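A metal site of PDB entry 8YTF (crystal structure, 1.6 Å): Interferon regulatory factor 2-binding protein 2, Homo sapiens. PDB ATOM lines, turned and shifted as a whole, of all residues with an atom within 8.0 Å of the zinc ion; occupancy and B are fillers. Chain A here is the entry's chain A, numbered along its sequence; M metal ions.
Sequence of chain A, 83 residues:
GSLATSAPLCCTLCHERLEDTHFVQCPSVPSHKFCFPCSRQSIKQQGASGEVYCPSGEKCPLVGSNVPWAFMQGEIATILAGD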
ATOM      1  N   THR A  12      -7.666   5.999  -3.393  1.00  0.00           N
ATOM      2  CA  THR A  12      -6.611   6.549  -4.231  1.00  0.00           C
ATOM      3  C   THR A  12      -6.646   5.969  -5.638  1.00  0.00           C
ATOM      4  O   THR A  12      -6.335   6.678  -6.609  1.00  0.00           O
ATOM      5  CB  THR A  12      -5.267   6.283  -3.544  1.00  0.00           C
ATOM      6  OG1 THR A  12      -5.222   7.016  -2.321  1.00  0.00           O
ATOM      7  CG2 THR A  12      -4.071   6.675  -4.417  1.00  0.00           C
ATOM      8  N   GLN A  25      -5.421   2.364   5.291  1.00  0.00           N
ATOM      9  CA  GLN A  25      -4.823   3.678   5.415  1.00  0.00           C
ATOM     10  C   GLN A  25      -3.314   3.549   5.448  1.00  0.00           C
ATOM     11  O   GLN A  25      -2.767   2.944   6.387  1.00  0.00           O
ATOM     12  CB  GLN A  25      -5.301   4.367   6.699  1.00  0.00           C
ATOM     13  CG  GLN A  25      -4.569   5.654   6.951  1.00  0.00           C
ATOM     14  CD  GLN A  25      -4.898   6.681   5.876  1.00  0.00           C
ATOM     15  OE1 GLN A  25      -6.054   7.058   5.720  1.00  0.00           O
ATOM     16  NE2 GLN A  25      -3.882   7.132   5.146  1.00  0.00           N
ATOM     17  N   CYS A  26      -2.645   4.099   4.444  1.00  0.00           N
ATOM     18  CA  CYS A  26      -1.192   4.189   4.486  1.00  0.00           C
ATOM     19  C   CYS A  26      -0.736   4.983   5.698  1.00  0.00           C
ATOM     20  O   CYS A  26      -1.200   6.117   5.901  1.00  0.00           O
ATOM     21  CB  CYS A  26      -0.698   4.871   3.214  1.00  0.00           C
ATOM     22  SG  CYS A  26       1.069   5.241   3.091  1.00  0.00           S
ATOM     23  N   PRO A  27       0.165   4.437   6.526  1.00  0.00           N
ATOM     24  CA  PRO A  27       0.574   5.143   7.757  1.00  0.00           C
ATOM     25  C   PRO A  27       1.192   6.525   7.537  1.00  0.00           C
ATOM     26  O   PRO A  27       0.994   7.419   8.365  1.00  0.00           O
ATOM     27  CB  PRO A  27       1.619   4.190   8.355  1.00  0.00           C
ATOM     28  CG  PRO A  27       1.261   2.857   7.831  1.00  0.00           C
ATOM     29  CD  PRO A  27       0.696   3.070   6.452  1.00  0.00           C
ATOM     30  N   SER A  28       1.970   6.708   6.473  1.00  0.00           N
ATOM     31  CA  SER A  28       2.791   7.906   6.328  1.00  0.00           C
ATOM     32  C   SER A  28       2.274   8.890   5.290  1.00  0.00           C
ATOM     33  O   SER A  28       2.813  10.016   5.182  1.00  0.00           O
ATOM     34  CB  SER A  28       4.239   7.534   6.002  1.00  0.00           C
ATOM     35  OG  SER A  28       4.316   6.575   4.960  1.00  0.00           O
ATOM     36  N   VAL A  29       1.252   8.532   4.523  1.00  0.00           N
ATOM     37  CA  VAL A  29       0.661   9.434   3.534  1.00  0.00           C
ATOM     38  C   VAL A  29      -0.846   9.486   3.777  1.00  0.00           C
ATOM     39  O   VAL A  29      -1.554   8.534   3.422  1.00  0.00           O
ATOM     40  CB  VAL A  29       0.976   8.975   2.104  1.00  0.00           C
ATOM     41  CG1 VAL A  29       0.400   9.967   1.089  1.00  0.00           C
ATOM     42  CG2 VAL A  29       2.463   8.841   1.915  1.00  0.00           C
ATOM     43  N   PRO A  30      -1.366  10.553   4.374  1.00  0.00           N
ATOM     44  CA  PRO A  30      -2.800  10.585   4.674  1.00  0.00           C
ATOM     45  C   PRO A  30      -3.680  10.338   3.469  1.00  0.00           C
ATOM     46  O   PRO A  30      -4.693   9.640   3.608  1.00  0.00           O
ATOM     47  CB  PRO A  30      -2.991  11.996   5.252  1.00  0.00           C
ATOM     48  CG  PRO A  30      -1.655  12.309   5.875  1.00  0.00           C
ATOM     49  CD  PRO A  30      -0.645  11.711   4.943  1.00  0.00           C
ATOM     50  N   SER A  31      -3.322  10.856   2.290  1.00  0.00           N
ATOM     51  CA  SER A  31      -4.207  10.722   1.136  1.00  0.00           C
ATOM     52  C   SER A  31      -4.188   9.329   0.518  1.00  0.00           C
ATOM     53  O   SER A  31      -5.016   9.064  -0.363  1.00  0.00           O
ATOM     54  CB  SER A  31      -3.824  11.754   0.067  1.00  0.00           C
ATOM     55  OG  SER A  31      -2.530  11.489  -0.429  1.00  0.00           O
ATOM     56  N   HIS A  32      -3.278   8.448   0.931  1.00  0.00           N
ATOM     57  CA  HIS A  32      -3.229   7.073   0.407  1.00  0.00           C
ATOM     58  C   HIS A  32      -4.229   6.229   1.173  1.00  0.00           C
ATOM     59  O   HIS A  32      -3.942   5.751   2.276  1.00  0.00           O
ATOM     60  CB  HIS A  32      -1.840   6.483   0.569  1.00  0.00           C
ATOM     61  CG  HIS A  32      -0.864   6.943  -0.454  1.00  0.00           C
ATOM     62  ND1 HIS A  32       0.445   6.531  -0.451  1.00  0.00           N
ATOM     63  CD2 HIS A  32      -1.002   7.788  -1.507  1.00  0.00           C
ATOM     64  CE1 HIS A  32       1.087   7.105  -1.463  1.00  0.00           C
ATOM     65  NE2 HIS A  32       0.228   7.867  -2.122  1.00  0.00           N
ATOM     66  N   LYS A  33      -5.412   6.031   0.582  1.00  0.00           N
ATOM     67  CA  LYS A  33      -6.510   5.278   1.166  1.00  0.00           C
ATOM     68  C   LYS A  33      -6.998   4.280   0.126  1.00  0.00           C
ATOM     69  O   LYS A  33      -7.171   4.640  -1.037  1.00  0.00           O
ATOM     70  CB  LYS A  33      -7.649   6.201   1.586  1.00  0.00           C
ATOM     71  CG  LYS A  33      -7.229   7.362   2.478  1.00  0.00           C
ATOM     72  CD  LYS A  33      -8.428   8.275   2.809  1.00  0.00           C
ATOM     73  CE  LYS A  33      -7.962   9.581   3.446  1.00  0.00           C
ATOM     74  NZ  LYS A  33      -7.364   9.408   4.798  1.00  0.00           N
ATOM     75  N   PHE A  34      -7.190   3.029   0.525  1.00  0.00           N
ATOM     76  CA  PHE A  34      -7.510   1.988  -0.447  1.00  0.00           C
ATOM     77  C   PHE A  34      -8.666   1.136   0.036  1.00  0.00           C
ATOM     78  O   PHE A  34      -8.623   0.578   1.130  1.00  0.00           O
ATOM     79  CB  PHE A  34      -6.292   1.119  -0.755  1.00  0.00           C
ATOM     80  CG  PHE A  34      -5.053   1.917  -1.004  1.00  0.00           C
ATOM     81  CD1 PHE A  34      -4.792   2.429  -2.269  1.00  0.00           C
ATOM     82  CD2 PHE A  34      -4.166   2.204   0.032  1.00  0.00           C
ATOM     83  CE1 PHE A  34      -3.656   3.194  -2.497  1.00  0.00           C
ATOM     84  CE2 PHE A  34      -3.030   2.969  -0.195  1.00  0.00           C
ATOM     85  CZ  PHE A  34      -2.783   3.456  -1.462  1.00  0.00           C
ATOM     86  N   TYR A  53       3.715  -3.939  -0.012  1.00  0.00           N
ATOM     87  CA  TYR A  53       3.943  -2.576   0.422  1.00  0.00           C
ATOM     88  C   TYR A  53       2.717  -1.725   0.088  1.00  0.00           C
ATOM     89  O   TYR A  53       1.699  -2.251  -0.390  1.00  0.00           O
ATOM     90  CB  TYR A  53       5.208  -2.034  -0.241  1.00  0.00           C
ATOM     91  CG  TYR A  53       6.451  -2.805   0.095  1.00  0.00           C
ATOM     92  CD1 TYR A  53       6.643  -3.312   1.352  1.00  0.00           C
ATOM     93  CD2 TYR A  53       7.428  -3.032  -0.865  1.00  0.00           C
ATOM     94  CE1 TYR A  53       7.752  -4.019   1.633  1.00  0.00           C
ATOM     95  CE2 TYR A  53       8.593  -3.750  -0.550  1.00  0.00           C
ATOM     96  CZ  TYR A  53       8.746  -4.219   0.711  1.00  0.00           C
ATOM     97  OH  TYR A  53       9.890  -4.935   1.072  1.00  0.00           O
ATOM     98  N   CYS A  54       2.822  -0.417   0.304  1.00  0.00           N
ATOM     99  CA  CYS A  54       1.679   0.470   0.065  1.00  0.00           C
ATOM    100  C   CYS A  54       1.138   0.257  -1.347  1.00  0.00           C
ATOM    101  O   CYS A  54       1.911   0.226  -2.315  1.00  0.00           O
ATOM    102  CB  CYS A  54       2.073   1.936   0.239  1.00  0.00           C
ATOM    103  SG  CYS A  54       0.687   3.072  -0.113  1.00  0.00           S
ATOM    104  N   PRO A  55      -0.179   0.107  -1.510  1.00  0.00           N
ATOM    105  CA  PRO A  55      -0.727  -0.106  -2.857  1.00  0.00           C
ATOM    106  C   PRO A  55      -0.459   1.019  -3.848  1.00  0.00           C
ATOM    107  O   PRO A  55      -0.625   0.793  -5.063  1.00  0.00           O
ATOM    108  CB  PRO A  55      -2.238  -0.264  -2.599  1.00  0.00           C
ATOM    109  CG  PRO A  55      -2.265  -0.905  -1.243  1.00  0.00           C
ATOM    110  CD  PRO A  55      -1.186  -0.149  -0.472  1.00  0.00           C
ATOM    111  N   SER A  56      -0.028   2.210  -3.400  1.00  0.00           N
ATOM    112  CA  SER A  56       0.365   3.261  -4.329  1.00  0.00           C
ATOM    113  C   SER A  56       1.578   2.867  -5.152  1.00  0.00           C
ATOM    114  O   SER A  56       1.838   3.494  -6.178  1.00  0.00           O
ATOM    115  CB  SER A  56       0.725   4.529  -3.588  1.00  0.00           C
ATOM    116  OG  SER A  56       1.856   4.285  -2.755  1.00  0.00           O
ATOM    117  N   GLY A  57       2.345   1.877  -4.698  1.00  0.00           N
ATOM    118  CA  GLY A  57       3.611   1.545  -5.309  1.00  0.00           C
ATOM    119  C   GLY A  57       4.769   2.445  -4.940  1.00  0.00           C
ATOM    120  O   GLY A  57       5.877   2.228  -5.444  1.00  0.00           O
ATOM    121  N   GLU A  58       4.555   3.436  -4.074  1.00  0.00           N
ATOM    122  CA  GLU A  58       5.594   4.390  -3.736  1.00  0.00           C
ATOM    123  C   GLU A  58       6.458   3.948  -2.557  1.00  0.00           C
ATOM    124  O   GLU A  58       7.351   4.703  -2.157  1.00  0.00           O
ATOM    125  CB  GLU A  58       4.976   5.760  -3.454  1.00  0.00           C
ATOM    126  CG  GLU A  58       4.239   6.271  -4.685  1.00  0.00           C
ATOM    127  CD  GLU A  58       3.476   7.557  -4.473  1.00  0.00           C
ATOM    128  OE1 GLU A  58       3.585   8.165  -3.395  1.00  0.00           O
ATOM    129  OE2 GLU A  58       2.779   7.955  -5.433  1.00  0.00           O
ATOM    130  N   LYS A  59       6.224   2.752  -2.008  1.00  0.00           N
ATOM    131  CA  LYS A  59       7.036   2.207  -0.915  1.00  0.00           C
ATOM    132  C   LYS A  59       7.123   3.178   0.262  1.00  0.00           C
ATOM    133  O   LYS A  59       8.193   3.425   0.836  1.00  0.00           O
ATOM    134  CB  LYS A  59       8.417   1.803  -1.422  1.00  0.00           C
ATOM    135  CG  LYS A  59       8.281   0.782  -2.530  1.00  0.00           C
ATOM    136  CD  LYS A  59       9.614   0.299  -3.022  1.00  0.00           C
ATOM    137  CE  LYS A  59       9.498  -0.135  -4.462  1.00  0.00           C
ATOM    138  NZ  LYS A  59      10.575  -1.086  -4.804  1.00  0.00           N
ATOM    139  N   CYS A  60       5.960   3.695   0.639  1.00  0.00           N
ATOM    140  CA  CYS A  60       5.862   4.672   1.712  1.00  0.00           C
ATOM    141  C   CYS A  60       6.412   4.098   3.018  1.00  0.00           C
ATOM    142  O   CYS A  60       6.221   2.903   3.299  1.00  0.00           O
ATOM    143  CB  CYS A  60       4.412   5.111   1.892  1.00  0.00           C
ATOM    144  SG  CYS A  60       3.623   5.409   0.288  1.00  0.00           S
ATOM    145  N   PRO A  61       7.095   4.889   3.819  1.00  0.00           N
ATOM    146  CA  PRO A  61       7.735   4.361   5.024  1.00  0.00           C
ATOM    147  C   PRO A  61       6.754   4.069   6.132  1.00  0.00           C
ATOM    148  O   PRO A  61       5.689   4.686   6.247  1.00  0.00           O
ATOM    149  CB  PRO A  61       8.690   5.487   5.438  1.00  0.00           C
ATOM    150  CG  PRO A  61       8.021   6.734   4.928  1.00  0.00           C
ATOM    151  CD  PRO A  61       7.391   6.321   3.609  1.00  0.00           C
ATOM    152  N   TRP A  69       6.541   0.402   4.869  1.00  0.00           N
ATOM    153  CA  TRP A  69       5.628  -0.419   5.654  1.00  0.00           C
ATOM    154  C   TRP A  69       5.090  -1.573   4.811  1.00  0.00           C
ATOM    155  O   TRP A  69       4.895  -1.449   3.599  1.00  0.00           O
ATOM    156  CB  TRP A  69       4.477   0.412   6.218  1.00  0.00           C
ATOM    157  CG  TRP A  69       3.486   0.921   5.210  1.00  0.00           C
ATOM    158  CD1 TRP A  69       3.502   2.140   4.593  1.00  0.00           C
ATOM    159  CD2 TRP A  69       2.301   0.269   4.764  1.00  0.00           C
ATOM    160  NE1 TRP A  69       2.409   2.273   3.761  1.00  0.00           N
ATOM    161  CE2 TRP A  69       1.652   1.124   3.859  1.00  0.00           C
ATOM    162  CE3 TRP A  69       1.719  -0.975   5.052  1.00  0.00           C
ATOM    163  CZ2 TRP A  69       0.442   0.790   3.229  1.00  0.00           C
ATOM    164  CZ3 TRP A  69       0.520  -1.316   4.429  1.00  0.00           C
ATOM    165  CH2 TRP A  69      -0.097  -0.437   3.512  1.00  0.00           C
HETATM  166 ZN    ZN M   1       1.417   5.124   0.767  1.00  0.00          ZN
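The backbone carbonyl oxygen (O) of His 32 is in hydrogen-bond range of the side-chain amide nitrogen (NE2) of Gln 25, at 3.2 Å.
The side-chain hydroxyl (OG) of Ser 56 sits close to the side-chain sulfur (SG) of Cys 60 (3.7 Å).
The backbone NH (N) of Trp 69 lies within hydrogen-bond range of the backbone carbonyl oxygen (O) of Cys 60.
SG of Cys 54 lies close to OG of Ser 56.
The side-chain sulfur (SG) of Cys 26 lies close to the backbone NH (N) of Val 29, at 3.6 Å.
The side-chain sulfur of Cys 26 lies close to the indole nitrogen of Trp 69 (3.3 Å).
The side-chain sulfur of Cys 26 sits close to the backbone NH of Ser 28, 3.8 Å away.
The side-chain hydroxyl (OG) of Ser 56 is in hydrogen-bond range of the backbone NH (N) of Glu 58.
OG of Ser 56 touches the zinc ion (3.6 Å).
Within 4 Å of the zinc ion: Cys 26, His 32, Cys 54, Ser 56 and Cys 60.
Along chain A the residues within 4 Å of the zinc ion span positions 26 to 60.
The nearest printed residue that does not touch the zinc ion is Val 29 (4.03 Å).
The zinc ion is bound by ND1 of His 32 (2.1 Å), SG of Cys 60 (2.3 Å), SG of Cys 54 (2.3 Å) and SG of Cys 26 (2.4 Å).
The zinc ion has four donor atoms within binding distance.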
